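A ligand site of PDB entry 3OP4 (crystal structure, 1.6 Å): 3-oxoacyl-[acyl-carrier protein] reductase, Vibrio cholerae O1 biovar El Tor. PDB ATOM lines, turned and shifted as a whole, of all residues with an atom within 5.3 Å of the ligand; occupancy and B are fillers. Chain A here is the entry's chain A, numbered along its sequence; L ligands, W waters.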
ATOM      1  N   THR A  15     -19.928  21.690 -30.535  1.00  0.00           N
ATOM      2  CA  THR A  15     -19.032  21.286 -29.420  1.00  0.00           C
ATOM      3  C   THR A  15     -19.149  19.770 -29.176  1.00  0.00           C
ATOM      4  O   THR A  15     -20.252  19.246 -29.175  1.00  0.00           O
ATOM      5  CB  THR A  15     -19.297  22.111 -28.135  1.00  0.00           C
ATOM      6  OG1 THR A  15     -20.618  21.850 -27.636  1.00  0.00           O
ATOM      7  CG2 THR A  15     -19.162  23.637 -28.401  1.00  0.00           C
ATOM      8  N   GLY A  16     -18.036  19.089 -28.932  1.00  0.00           N
ATOM      9  CA  GLY A  16     -18.032  17.640 -28.666  1.00  0.00           C
ATOM     10  C   GLY A  16     -18.482  16.884 -29.868  1.00  0.00           C
ATOM     11  O   GLY A  16     -19.443  16.088 -29.807  1.00  0.00           O
ATOM     12  N   ALA A  17     -17.694  17.038 -30.950  1.00  0.00           N
ATOM     13  CA  ALA A  17     -17.961  16.395 -32.228  1.00  0.00           C
ATOM     14  C   ALA A  17     -17.047  15.226 -32.566  1.00  0.00           C
ATOM     15  O   ALA A  17     -17.097  14.683 -33.672  1.00  0.00           O
ATOM     16  CB  ALA A  17     -17.991  17.457 -33.382  1.00  0.00           C
ATOM     17  N   SER A  18     -16.330  14.735 -31.582  1.00  0.00           N
ATOM     18  CA  SER A  18     -15.399  13.643 -31.791  1.00  0.00           C
ATOM     19  C   SER A  18     -16.085  12.281 -31.891  1.00  0.00           C
ATOM     20  O   SER A  18     -15.522  11.352 -32.492  1.00  0.00           O
ATOM     21  CB  SER A  18     -14.323  13.641 -30.689  1.00  0.00           C
ATOM     22  OG  SER A  18     -14.949  13.665 -29.410  1.00  0.00           O
ATOM     23  N   ARG A  19     -17.279  12.161 -31.312  1.00  0.00           N
ATOM     24  CA  ARG A  19     -18.000  10.886 -31.235  1.00  0.00           C
ATOM     25  C   ARG A  19     -19.452  11.164 -30.881  1.00  0.00           C
ATOM     26  O   ARG A  19     -19.810  12.295 -30.584  1.00  0.00           O
ATOM     27  CB  ARG A  19     -17.339   9.985 -30.173  1.00  0.00           C
ATOM     28  CG  ARG A  19     -17.253  10.676 -28.787  1.00  0.00           C
ATOM     29  CD  ARG A  19     -16.371   9.896 -27.801  1.00  0.00           C
ATOM     30  NE  ARG A  19     -16.023  10.700 -26.631  1.00  0.00           N
ATOM     31  CZ  ARG A  19     -16.295  10.403 -25.380  1.00  0.00           C
ATOM     32  NH1 ARG A  19     -16.907   9.262 -25.059  1.00  0.00           N
ATOM     33  NH2 ARG A  19     -15.924  11.244 -24.438  1.00  0.00           N
ATOM     34  N   GLY A  20     -20.264  10.106 -30.883  1.00  0.00           N
ATOM     35  CA  GLY A  20     -21.591  10.207 -30.435  1.00  0.00           C
ATOM     36  C   GLY A  20     -22.483  11.156 -31.267  1.00  0.00           C
ATOM     37  O   GLY A  20     -22.415  11.295 -32.496  1.00  0.00           O
ATOM     38  N   ILE A  21     -23.385  11.779 -30.522  1.00  0.00           N
ATOM     39  CA  ILE A  21     -24.360  12.696 -31.096  1.00  0.00           C
ATOM     40  C   ILE A  21     -23.711  13.894 -31.781  1.00  0.00           C
ATOM     41  O   ILE A  21     -24.088  14.244 -32.864  1.00  0.00           O
ATOM     42  CB  ILE A  21     -25.356  13.176 -30.005  1.00  0.00           C
ATOM     43  CG1 ILE A  21     -26.291  12.025 -29.579  1.00  0.00           C
ATOM     44  CG2 ILE A  21     -26.140  14.438 -30.461  1.00  0.00           C
ATOM     45  CD1 ILE A  21     -26.968  12.276 -28.248  1.00  0.00           C
ATOM     46  N   GLY A  22     -22.680  14.450 -31.160  1.00  0.00           N
ATOM     47  CA  GLY A  22     -22.011  15.605 -31.756  1.00  0.00           C
ATOM     48  C   GLY A  22     -21.354  15.297 -33.098  1.00  0.00           C
ATOM     49  O   GLY A  22     -21.382  16.134 -34.011  1.00  0.00           O
ATOM     50  N   THR A  39     -15.524  20.237 -32.241  1.00  0.00           N
ATOM     51  CA  THR A  39     -14.508  20.277 -31.189  1.00  0.00           C
ATOM     52  C   THR A  39     -14.365  18.973 -30.417  1.00  0.00           C
ATOM     53  O   THR A  39     -15.283  18.168 -30.272  1.00  0.00           O
ATOM     54  CB  THR A  39     -14.714  21.440 -30.214  1.00  0.00           C
ATOM     55  OG1 THR A  39     -15.761  21.139 -29.295  1.00  0.00           O
ATOM     56  CG2 THR A  39     -14.974  22.772 -30.943  1.00  0.00           C
ATOM     57  N   ALA A  40     -13.150  18.747 -29.923  1.00  0.00           N
ATOM     58  CA  ALA A  40     -12.874  17.665 -28.962  1.00  0.00           C
ATOM     59  C   ALA A  40     -12.044  18.225 -27.809  1.00  0.00           C
ATOM     60  O   ALA A  40     -11.514  19.322 -27.941  1.00  0.00           O
ATOM     61  CB  ALA A  40     -12.114  16.490 -29.647  1.00  0.00           C
ATOM     62  N   THR A  41     -11.943  17.496 -26.709  1.00  0.00           N
ATOM     63  CA  THR A  41     -11.123  17.946 -25.589  1.00  0.00           C
ATOM     64  C   THR A  41      -9.650  17.667 -25.851  1.00  0.00           C
ATOM     65  O   THR A  41      -8.821  18.270 -25.162  1.00  0.00           O
ATOM     66  CB  THR A  41     -11.487  17.318 -24.243  1.00  0.00           C
ATOM     67  OG1 THR A  41     -11.260  15.917 -24.295  1.00  0.00           O
ATOM     68  CG2 THR A  41     -13.021  17.546 -23.913  1.00  0.00           C
ATOM     69  N   SER A  42      -9.339  16.819 -26.846  1.00  0.00           N
ATOM     70  CA  SER A  42      -7.934  16.410 -27.128  1.00  0.00           C
ATOM     71  C   SER A  42      -7.497  16.802 -28.544  1.00  0.00           C
ATOM     72  O   SER A  42      -8.342  16.996 -29.439  1.00  0.00           O
ATOM     73  CB  SER A  42      -7.833  14.870 -27.017  1.00  0.00           C
ATOM     74  OG  SER A  42      -8.577  14.283 -28.062  1.00  0.00           O
ATOM     75  N   LEU A  62     -11.195  22.195 -27.599  1.00  0.00           N
ATOM     76  CA  LEU A  62     -11.991  23.128 -26.782  1.00  0.00           C
ATOM     77  C   LEU A  62     -12.374  22.382 -25.508  1.00  0.00           C
ATOM     78  O   LEU A  62     -12.853  21.224 -25.547  1.00  0.00           O
ATOM     79  CB  LEU A  62     -13.310  23.477 -27.471  1.00  0.00           C
ATOM     80  CG  LEU A  62     -14.281  24.307 -26.651  1.00  0.00           C
ATOM     81  CD1 LEU A  62     -13.707  25.684 -26.282  1.00  0.00           C
ATOM     82  CD2 LEU A  62     -15.540  24.431 -27.565  1.00  0.00           C
ATOM     83  N   ASN A  63     -12.160  23.034 -24.355  1.00  0.00           N
ATOM     84  CA  ASN A  63     -12.758  22.624 -23.113  1.00  0.00           C
ATOM     85  C   ASN A  63     -13.766  23.702 -22.722  1.00  0.00           C
ATOM     86  O   ASN A  63     -13.407  24.857 -22.452  1.00  0.00           O
ATOM     87  CB  ASN A  63     -11.710  22.441 -22.012  1.00  0.00           C
ATOM     88  CG  ASN A  63     -12.308  21.814 -20.774  1.00  0.00           C
ATOM     89  OD1 ASN A  63     -13.459  22.062 -20.438  1.00  0.00           O
ATOM     90  ND2 ASN A  63     -11.542  20.934 -20.119  1.00  0.00           N
ATOM     91  N   VAL A  64     -15.060  23.328 -22.730  1.00  0.00           N
ATOM     92  CA  VAL A  64     -16.092  24.304 -22.484  1.00  0.00           C
ATOM     93  C   VAL A  64     -16.200  24.782 -21.046  1.00  0.00           C
ATOM     94  O   VAL A  64     -16.967  25.702 -20.814  1.00  0.00           O
ATOM     95  CB  VAL A  64     -17.510  23.818 -22.943  1.00  0.00           C
ATOM     96  CG1 VAL A  64     -17.494  23.452 -24.413  1.00  0.00           C
ATOM     97  CG2 VAL A  64     -18.029  22.633 -22.086  1.00  0.00           C
ATOM     98  N   THR A  65     -15.401  24.232 -20.132  1.00  0.00           N
ATOM     99  CA  THR A  65     -15.333  24.744 -18.746  1.00  0.00           C
ATOM    100  C   THR A  65     -14.243  25.790 -18.572  1.00  0.00           C
ATOM    101  O   THR A  65     -14.097  26.312 -17.450  1.00  0.00           O
ATOM    102  CB  THR A  65     -15.128  23.611 -17.707  1.00  0.00           C
ATOM    103  OG1 THR A  65     -13.823  23.034 -17.842  1.00  0.00           O
ATOM    104  CG2 THR A  65     -16.146  22.502 -17.838  1.00  0.00           C
ATOM    105  N   ASN A  89     -24.664  23.517 -28.879  1.00  0.00           N
ATOM    106  CA  ASN A  89     -24.070  23.209 -27.605  1.00  0.00           C
ATOM    107  C   ASN A  89     -24.348  21.749 -27.222  1.00  0.00           C
ATOM    108  O   ASN A  89     -25.322  21.431 -26.532  1.00  0.00           O
ATOM    109  CB  ASN A  89     -24.600  24.144 -26.528  1.00  0.00           C
ATOM    110  CG  ASN A  89     -24.056  25.549 -26.621  1.00  0.00           C
ATOM    111  OD1 ASN A  89     -22.814  25.758 -26.738  1.00  0.00           O
ATOM    112  ND2 ASN A  89     -24.948  26.534 -26.596  1.00  0.00           N
ATOM    113  N   ASN A  90     -23.484  20.903 -27.667  1.00  0.00           N
ATOM    114  CA  ASN A  90     -23.611  19.437 -27.533  1.00  0.00           C
ATOM    115  C   ASN A  90     -22.741  18.893 -26.426  1.00  0.00           C
ATOM    116  O   ASN A  90     -23.122  17.948 -25.757  1.00  0.00           O
ATOM    117  CB  ASN A  90     -23.375  18.711 -28.876  1.00  0.00           C
ATOM    118  CG  ASN A  90     -23.255  17.233 -28.724  1.00  0.00           C
ATOM    119  OD1 ASN A  90     -24.276  16.534 -28.691  1.00  0.00           O
ATOM    120  ND2 ASN A  90     -22.021  16.716 -28.616  1.00  0.00           N
ATOM    121  N   ALA A  91     -21.539  19.442 -26.206  1.00  0.00           N
ATOM    122  CA  ALA A  91     -20.686  18.936 -25.156  1.00  0.00           C
ATOM    123  C   ALA A  91     -21.369  18.773 -23.826  1.00  0.00           C
ATOM    124  O   ALA A  91     -22.071  19.681 -23.378  1.00  0.00           O
ATOM    125  CB  ALA A  91     -19.435  19.827 -24.982  1.00  0.00           C
ATOM    126  N   GLY A  92     -21.249  17.591 -23.217  1.00  0.00           N
ATOM    127  CA  GLY A  92     -21.801  17.375 -21.915  1.00  0.00           C
ATOM    128  C   GLY A  92     -21.338  16.036 -21.383  1.00  0.00           C
ATOM    129  O   GLY A  92     -20.830  15.179 -22.108  1.00  0.00           O
ATOM    130  N   ILE A  93     -21.484  15.886 -20.073  1.00  0.00           N
ATOM    131  CA  ILE A  93     -21.021  14.718 -19.336  1.00  0.00           C
ATOM    132  C   ILE A  93     -22.061  14.276 -18.282  1.00  0.00           C
ATOM    133  O   ILE A  93     -22.993  14.989 -18.050  1.00  0.00           O
ATOM    134  CB  ILE A  93     -19.707  15.012 -18.563  1.00  0.00           C
ATOM    135  CG1 ILE A  93     -19.864  16.238 -17.638  1.00  0.00           C
ATOM    136  CG2 ILE A  93     -18.558  15.251 -19.600  1.00  0.00           C
ATOM    137  CD1 ILE A  93     -18.672  16.424 -16.646  1.00  0.00           C
ATOM    138  N   THR A 113     -19.926  22.033 -16.754  1.00  0.00           N
ATOM    139  CA  THR A 113     -19.814  21.432 -18.080  1.00  0.00           C
ATOM    140  C   THR A 113     -21.122  21.492 -18.832  1.00  0.00           C
ATOM    141  O   THR A 113     -21.118  21.702 -20.065  1.00  0.00           O
ATOM    142  CB  THR A 113     -19.318  19.947 -18.009  1.00  0.00           C
ATOM    143  OG1 THR A 113     -18.134  19.899 -17.171  1.00  0.00           O
ATOM    144  CG2 THR A 113     -18.979  19.326 -19.388  1.00  0.00           C
ATOM    145  N   ASN A 114     -22.249  21.345 -18.125  1.00  0.00           N
ATOM    146  CA  ASN A 114     -23.542  21.107 -18.836  1.00  0.00           C
ATOM    147  C   ASN A 114     -24.441  22.346 -18.824  1.00  0.00           C
ATOM    148  O   ASN A 114     -25.459  22.381 -19.554  1.00  0.00           O
ATOM    149  CB  ASN A 114     -24.317  19.921 -18.248  1.00  0.00           C
ATOM    150  CG  ASN A 114     -23.653  18.564 -18.509  1.00  0.00           C
ATOM    151  OD1 ASN A 114     -22.473  18.491 -18.935  1.00  0.00           O
ATOM    152  ND2 ASN A 114     -24.361  17.502 -18.225  1.00  0.00           N
ATOM    153  N   VAL A 140     -28.257  20.901 -26.818  1.00  0.00           N
ATOM    154  CA  VAL A 140     -28.636  19.481 -26.688  1.00  0.00           C
ATOM    155  C   VAL A 140     -28.951  19.261 -25.187  1.00  0.00           C
ATOM    156  O   VAL A 140     -28.069  19.254 -24.323  1.00  0.00           O
ATOM    157  CB  VAL A 140     -27.544  18.501 -27.196  1.00  0.00           C
ATOM    158  CG1 VAL A 140     -28.026  17.035 -26.989  1.00  0.00           C
ATOM    159  CG2 VAL A 140     -27.137  18.777 -28.653  1.00  0.00           C
ATOM    160  N   GLY A 141     -30.241  19.100 -24.917  1.00  0.00           N
ATOM    161  CA  GLY A 141     -30.757  18.804 -23.581  1.00  0.00           C
ATOM    162  C   GLY A 141     -30.814  17.295 -23.357  1.00  0.00           C
ATOM    163  O   GLY A 141     -29.923  16.579 -23.793  1.00  0.00           O
ATOM    164  N   SER A 142     -31.848  16.860 -22.629  1.00  0.00           N
ATOM    165  CA  SER A 142     -32.095  15.445 -22.375  1.00  0.00           C
ATOM    166  C   SER A 142     -33.501  15.259 -21.890  1.00  0.00           C
ATOM    167  O   SER A 142     -34.050  16.117 -21.177  1.00  0.00           O
ATOM    168  CB  SER A 142     -31.217  14.917 -21.240  1.00  0.00           C
ATOM    169  OG  SER A 142     -31.513  13.547 -20.974  1.00  0.00           O
ATOM    170  N   VAL A 143     -34.112  14.144 -22.254  1.00  0.00           N
ATOM    171  CA  VAL A 143     -35.387  13.690 -21.670  1.00  0.00           C
ATOM    172  C   VAL A 143     -35.290  13.770 -20.129  1.00  0.00           C
ATOM    173  O   VAL A 143     -36.286  14.069 -19.484  1.00  0.00           O
ATOM    174  CB  VAL A 143     -35.771  12.272 -22.119  1.00  0.00           C
ATOM    175  CG1 VAL A 143     -34.804  11.180 -21.596  1.00  0.00           C
ATOM    176  CG2 VAL A 143     -37.243  11.997 -21.783  1.00  0.00           C
ATOM    177  N   TYR A 155     -27.295  16.117 -13.222  1.00  0.00           N
ATOM    178  CA  TYR A 155     -27.539  16.122 -14.659  1.00  0.00           C
ATOM    179  C   TYR A 155     -28.894  16.675 -15.019  1.00  0.00           C
ATOM    180  O   TYR A 155     -29.036  17.523 -15.927  1.00  0.00           O
ATOM    181  CB  TYR A 155     -27.394  14.699 -15.165  1.00  0.00           C
ATOM    182  CG  TYR A 155     -27.477  14.487 -16.653  1.00  0.00           C
ATOM    183  CD1 TYR A 155     -26.367  14.724 -17.478  1.00  0.00           C
ATOM    184  CD2 TYR A 155     -28.590  13.991 -17.255  1.00  0.00           C
ATOM    185  CE1 TYR A 155     -26.438  14.449 -18.863  1.00  0.00           C
ATOM    186  CE2 TYR A 155     -28.631  13.722 -18.580  1.00  0.00           C
ATOM    187  CZ  TYR A 155     -27.538  13.941 -19.372  1.00  0.00           C
ATOM    188  OH  TYR A 155     -27.574  13.698 -20.732  1.00  0.00           O
ATOM    189  N   LYS A 159     -29.683  20.006 -17.215  1.00  0.00           N
ATOM    190  CA  LYS A 159     -30.433  19.887 -18.471  1.00  0.00           C
ATOM    191  C   LYS A 159     -31.776  20.672 -18.403  1.00  0.00           C
ATOM    192  O   LYS A 159     -32.175  21.256 -19.425  1.00  0.00           O
ATOM    193  CB  LYS A 159     -30.661  18.401 -18.823  1.00  0.00           C
ATOM    194  CG  LYS A 159     -29.356  17.646 -19.212  1.00  0.00           C
ATOM    195  CD  LYS A 159     -28.627  18.283 -20.418  1.00  0.00           C
ATOM    196  CE  LYS A 159     -27.626  17.297 -20.978  1.00  0.00           C
ATOM    197  NZ  LYS A 159     -26.875  17.871 -22.152  1.00  0.00           N
ATOM    198  N   PRO A 185     -32.833  14.660 -26.521  1.00  0.00           N
ATOM    199  CA  PRO A 185     -32.831  13.193 -26.830  1.00  0.00           C
ATOM    200  C   PRO A 185     -33.276  12.339 -25.692  1.00  0.00           C
ATOM    201  O   PRO A 185     -33.102  12.707 -24.533  1.00  0.00           O
ATOM    202  CB  PRO A 185     -31.346  12.903 -27.110  1.00  0.00           C
ATOM    203  CG  PRO A 185     -30.732  14.260 -27.255  1.00  0.00           C
ATOM    204  CD  PRO A 185     -31.473  15.173 -26.382  1.00  0.00           C
ATOM    205  N   GLY A 186     -33.940  11.238 -26.039  1.00  0.00           N
ATOM    206  CA  GLY A 186     -34.100  10.089 -25.179  1.00  0.00           C
ATOM    207  C   GLY A 186     -32.797   9.310 -25.107  1.00  0.00           C
ATOM    208  O   GLY A 186     -31.708   9.900 -25.363  1.00  0.00           O
ATOM    209  N   PHE A 187     -32.863   8.014 -24.838  1.00  0.00           N
ATOM    210  CA  PHE A 187     -31.649   7.222 -24.806  1.00  0.00           C
ATOM    211  C   PHE A 187     -31.168   6.874 -26.196  1.00  0.00           C
ATOM    212  O   PHE A 187     -31.890   6.288 -27.018  1.00  0.00           O
ATOM    213  CB  PHE A 187     -31.842   5.979 -23.921  1.00  0.00           C
ATOM    214  CG  PHE A 187     -31.856   6.330 -22.418  1.00  0.00           C
ATOM    215  CD1 PHE A 187     -30.763   6.115 -21.615  1.00  0.00           C
ATOM    216  CD2 PHE A 187     -32.972   6.897 -21.831  1.00  0.00           C
ATOM    217  CE1 PHE A 187     -30.773   6.493 -20.259  1.00  0.00           C
ATOM    218  CE2 PHE A 187     -32.968   7.259 -20.462  1.00  0.00           C
ATOM    219  CZ  PHE A 187     -31.871   7.068 -19.703  1.00  0.00           C
ATOM    220  N   ILE A 188     -29.937   7.301 -26.472  1.00  0.00           N
ATOM    221  CA  ILE A 188     -29.324   7.235 -27.796  1.00  0.00           C
ATOM    222  C   ILE A 188     -28.119   6.324 -27.673  1.00  0.00           C
ATOM    223  O   ILE A 188     -27.353   6.402 -26.674  1.00  0.00           O
ATOM    224  CB  ILE A 188     -28.889   8.614 -28.283  1.00  0.00           C
ATOM    225  CG1 ILE A 188     -29.999   9.625 -28.166  1.00  0.00           C
ATOM    226  CG2 ILE A 188     -28.340   8.560 -29.711  1.00  0.00           C
ATOM    227  CD1 ILE A 188     -31.324   9.230 -28.852  1.00  0.00           C
ATOM    228  N   THR A 190     -24.741   5.591 -27.762  1.00  0.00           N
ATOM    229  CA  THR A 190     -23.416   6.239 -27.697  1.00  0.00           C
ATOM    230  C   THR A 190     -22.571   5.666 -26.555  1.00  0.00           C
ATOM    231  O   THR A 190     -23.031   4.767 -25.836  1.00  0.00           O
ATOM    232  CB  THR A 190     -23.521   7.759 -27.450  1.00  0.00           C
ATOM    233  OG1 THR A 190     -23.858   7.989 -26.067  1.00  0.00           O
ATOM    234  CG2 THR A 190     -24.600   8.403 -28.295  1.00  0.00           C
ATOM    235  N   ASP A 191     -21.378   6.211 -26.345  1.00  0.00           N
ATOM    236  CA  ASP A 191     -20.575   5.754 -25.203  1.00  0.00           C
ATOM    237  C   ASP A 191     -21.280   6.045 -23.849  1.00  0.00           C
ATOM    238  O   ASP A 191     -20.970   5.394 -22.818  1.00  0.00           O
ATOM    239  CB  ASP A 191     -19.216   6.437 -25.265  1.00  0.00           C
ATOM    240  CG  ASP A 191     -18.359   5.988 -26.447  1.00  0.00           C
ATOM    241  OD1 ASP A 191     -18.591   4.905 -27.030  1.00  0.00           O
ATOM    242  OD2 ASP A 191     -17.488   6.824 -26.780  1.00  0.00           O
ATOM    243  N   MET A 192     -22.148   7.065 -23.819  1.00  0.00           N
ATOM    244  CA  MET A 192     -22.772   7.464 -22.522  1.00  0.00           C
ATOM    245  C   MET A 192     -23.755   6.413 -22.125  1.00  0.00           C
ATOM    246  O   MET A 192     -23.891   6.034 -20.958  1.00  0.00           O
ATOM    247  CB  MET A 192     -23.463   8.846 -22.621  1.00  0.00           C
ATOM    248  CG  MET A 192     -24.110   9.373 -21.336  1.00  0.00           C
ATOM    249  SD  MET A 192     -24.795  11.210 -21.674  1.00  0.00           S
ATOM    250  CE  MET A 192     -23.042  12.176 -21.836  1.00  0.00           C
ATOM    251  N   THR A 193     -24.493   5.909 -23.112  1.00  0.00           N
ATOM    252  CA  THR A 193     -25.507   4.850 -22.907  1.00  0.00           C
ATOM    253  C   THR A 193     -24.792   3.565 -22.631  1.00  0.00           C
ATOM    254  O   THR A 193     -25.178   2.770 -21.745  1.00  0.00           O
ATOM    255  CB  THR A 193     -26.451   4.626 -24.139  1.00  0.00           C
ATOM    256  OG1 THR A 193     -27.697   4.066 -23.720  1.00  0.00           O
ATOM    257  CG2 THR A 193     -25.857   3.679 -25.172  1.00  0.00           C
HETATM  258  P1  LIG L   1     -20.299  11.217 -25.523  1.00  0.00           P
HETATM  259  O1  LIG L   1     -20.294  10.104 -26.471  1.00  0.00           O
HETATM  260  O2  LIG L   1     -19.834  11.066 -24.096  1.00  0.00           O
HETATM  261  O3  LIG L   1     -19.598  12.417 -26.186  1.00  0.00           O
HETATM  262  C1  LIG L   1     -19.336  13.620 -25.481  1.00  0.00           C
HETATM  263  C2  LIG L   1     -18.731  14.721 -26.322  1.00  0.00           C
HETATM  264  O4  LIG L   1     -18.546  15.903 -25.534  1.00  0.00           O
HETATM  265  C3  LIG L   1     -17.320  14.328 -26.759  1.00  0.00           C
HETATM  266  O5  LIG L   1     -17.030  14.864 -28.020  1.00  0.00           O
HETATM  267  C4  LIG L   1     -16.415  14.978 -25.701  1.00  0.00           C
HETATM  268  O6  LIG L   1     -15.049  15.222 -26.105  1.00  0.00           O
HETATM  269  C5  LIG L   1     -17.166  16.255 -25.448  1.00  0.00           C
HETATM  270  N1  LIG L   1     -16.888  16.783 -24.131  1.00  0.00           N
HETATM  271  C6  LIG L   1     -17.010  16.166 -22.924  1.00  0.00           C
HETATM  272  N2  LIG L   1     -16.606  17.045 -21.977  1.00  0.00           N
HETATM  273  C7  LIG L   1     -16.242  18.194 -22.579  1.00  0.00           C
HETATM  274  C8  LIG L   1     -15.709  19.410 -22.143  1.00  0.00           C
HETATM  275  N3  LIG L   1     -15.474  19.671 -20.832  1.00  0.00           N
HETATM  276  N4  LIG L   1     -15.421  20.408 -23.056  1.00  0.00           N
HETATM  277  C9  LIG L   1     -15.657  20.201 -24.416  1.00  0.00           C
HETATM  278  N5  LIG L   1     -16.108  18.988 -24.861  1.00  0.00           N
HETATM  279  C10 LIG L   1     -16.393  18.026 -23.975  1.00  0.00           C
HETATM  280  O7  LIG L   1     -21.782  11.828 -25.358  1.00  0.00           O
HETATM  281  P2  LIG L   1     -23.141  11.774 -26.183  1.00  0.00           P
HETATM  282  O8  LIG L   1     -22.874  11.820 -27.625  1.00  0.00           O
HETATM  283  O9  LIG L   1     -23.946  10.640 -25.676  1.00  0.00           O
HETATM  284  O10 LIG L   1     -23.739  13.170 -25.704  1.00  0.00           O
HETATM  285  C11 LIG L   1     -23.768  14.407 -26.391  1.00  0.00           C
HETATM  286  C12 LIG L   1     -24.782  15.254 -25.666  1.00  0.00           C
HETATM  287  O11 LIG L   1     -26.072  14.634 -25.724  1.00  0.00           O
HETATM  288  C13 LIG L   1     -24.502  15.552 -24.188  1.00  0.00           C
HETATM  289  O12 LIG L   1     -24.861  16.912 -23.879  1.00  0.00           O
HETATM  290  C14 LIG L   1     -25.428  14.586 -23.478  1.00  0.00           C
HETATM  291  O13 LIG L   1     -25.761  15.012 -22.159  1.00  0.00           O
HETATM  292  C15 LIG L   1     -26.611  14.629 -24.407  1.00  0.00           C
HETATM  293  N6  LIG L   1     -27.466  13.473 -24.333  1.00  0.00           N
HETATM  294  C16 LIG L   1     -27.058  12.185 -24.521  1.00  0.00           C
HETATM  295  C17 LIG L   1     -27.936  11.153 -24.479  1.00  0.00           C
HETATM  296  C18 LIG L   1     -27.568   9.749 -24.699  1.00  0.00           C
HETATM  297  O14 LIG L   1     -26.296   9.449 -25.166  1.00  0.00           O
HETATM  298  N7  LIG L   1     -28.404   8.827 -24.482  1.00  0.00           N
HETATM  299  C19 LIG L   1     -29.296  11.374 -24.195  1.00  0.00           C
HETATM  300  C20 LIG L   1     -29.688  12.684 -24.020  1.00  0.00           C
HETATM  301  C21 LIG L   1     -28.814  13.737 -24.056  1.00  0.00           C
HETATM  302  P3  LIG L   1     -13.991  14.001 -26.004  1.00  0.00           P
HETATM  303  O15 LIG L   1     -14.252  12.999 -27.099  1.00  0.00           O
HETATM  304  O16 LIG L   1     -14.059  13.369 -24.641  1.00  0.00           O
HETATM  305  O17 LIG L   1     -12.711  14.720 -26.257  1.00  0.00           O
HETATM  306  O   HOH W   1     -24.809  20.115 -23.964  1.00  0.00           O
HETATM  307  O   HOH W   2     -19.598   8.955 -22.424  1.00  0.00           O
HETATM  308  O   HOH W   3     -12.720  10.889 -27.749  1.00  0.00           O
HETATM  309  O   HOH W   4     -14.628  19.811 -27.217  1.00  0.00           O
HETATM  310  O   HOH W   5     -15.087  16.111 -19.763  1.00  0.00           O
HETATM  311  O   HOH W   6     -27.324   7.704 -21.648  1.00  0.00           O
HETATM  312  O   HOH W   7     -20.055   8.078 -28.049  1.00  0.00           O
HETATM  313  O   HOH W   8     -19.536  12.676 -22.038  1.00  0.00           O
HETATM  314  O   HOH W   9     -15.747  18.548 -18.102  1.00  0.00           O
HETATM  315  O   HOH W  10     -12.465  11.586 -23.834  1.00  0.00           O
HETATM  316  O   HOH W  11     -21.364  13.856 -28.674  1.00  0.00           O
HETATM  317  O   HOH W  12     -14.350  14.002 -22.117  1.00  0.00           O
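Water W7 lies within hydrogen-bond range of O1 of the ligand (2.6 Å), N of Asp 191 (2.9 Å) and N of Gly 20 (3.5 Å).
Water W8 bridges O2 of the ligand (2.6 Å) and O of Gly 92 (2.8 Å).
Water W3 lies within hydrogen-bond range of an oxygen (O15) of the ligand (2.7 Å) and the guanidinium group (NE) of Arg 19 (3.5 Å).
Water W2 bridges an oxygen (O2) of the ligand (2.7 Å) and the backbone NH of Met 192 (3.5 Å).
Water W9 bridges OG1 of Thr 113 (2.9 Å) and N3 of the ligand (3.0 Å).
OG1 of Thr 190 is in hydrogen-bond range of N of Met 192 (3.0 Å).
The side-chain amide nitrogen (ND2) of Asn 90 lies close to the backbone NH (N) of Gly 22, 3.5 Å away.
The backbone NH of Asn 90 lies within hydrogen-bond range of the side-chain hydroxyl of Thr 15 (3.0 Å).
The backbone NH (N) of Gly 16 is in hydrogen-bond range of the side-chain hydroxyl (OG1) of Thr 39.
The side-chain amide oxygen (OD1) of Asn 63 sits at hydrogen-bond distance from the side-chain hydroxyl (OG1) of Thr 65 (2.8 Å).
O of Asn 89 sits at hydrogen-bond distance from N of Val 140 (3.0 Å).
The backbone carbonyl oxygen (O) of Ile 93 sits at hydrogen-bond distance from the side-chain amide nitrogen (ND2) of Asn 114 (2.9 Å).
The backbone NH of Ala 17 is in hydrogen-bond range of the backbone carbonyl oxygen of Thr 39 (2.7 Å).
OG of Ser 18 sits at hydrogen-bond distance from O15 of the ligand (2.5 Å).
OH of Tyr 155 is in hydrogen-bond range of O13 of the ligand.
O9 of the ligand sits at hydrogen-bond distance from OG1 of Thr 190 (2.7 Å).
O17 of the ligand is in hydrogen-bond range of N of Thr 41, at 2.9 Å.
OG1 of Thr 41 lies within hydrogen-bond range of O17 of the ligand (2.7 Å).
An oxygen (O12) of the ligand lies within hydrogen-bond range of the backbone carbonyl oxygen (O) of Asn 90 (2.8 Å).
The side-chain amino group of Lys 159 lies within hydrogen-bond range of an oxygen (O12) of the ligand (2.8 Å).
NH2 of Arg 19 is in salt-bridge range of O16 of the ligand (2.8 Å).
The backbone carbonyl oxygen of Ile 188 sits at hydrogen-bond distance from a nitrogen (N7) of the ligand, 3.4 Å away.
The backbone NH of Ile 21 lies within hydrogen-bond range of an oxygen (O8) of the ligand.
The backbone NH (N) of Val 64 sits at hydrogen-bond distance from a nitrogen (N4) of the ligand (3.0 Å).
An oxygen (O5) of the ligand sits close to the backbone carbonyl oxygen (O) of Gly 16, 3.2 Å away.
N3 of the ligand is in hydrogen-bond range of OD1 of Asn 63 (3.2 Å).
Residues that only touch the ligand: Ala 17, Gly 20, Ala 40, Leu 62, Ala 91, Gly 92, Ile 93, Thr 113, Val 140, Gly 141, Ser 142, Pro 185, Gly 186, Phe 187 and Met 192.
Hydrophobic or aromatic side chains that line the ligand: Ile 21, Ala 40, Val 64, Ala 91, Ile 93, Val 140, Tyr 155, Pro 185, Ile 188 and Met 192.
27 residues have an atom within 4 Å of the ligand: Gly 16, Ala 17, Ser 18, Arg 19, Gly 20, Ile 21, Ala 40, Thr 41, Leu 62, Asn 63, Val 64, Asn 90, Ala 91, Gly 92, Ile 93, Thr 113, Val 140, Gly 141, Ser 142, Tyr 155, Lys 159, Pro 185, Gly 186, Phe 187, Ile 188, Thr 190 and Met 192.
The nearest printed residue that does not touch the ligand is Asp 191 (4.01 Å).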
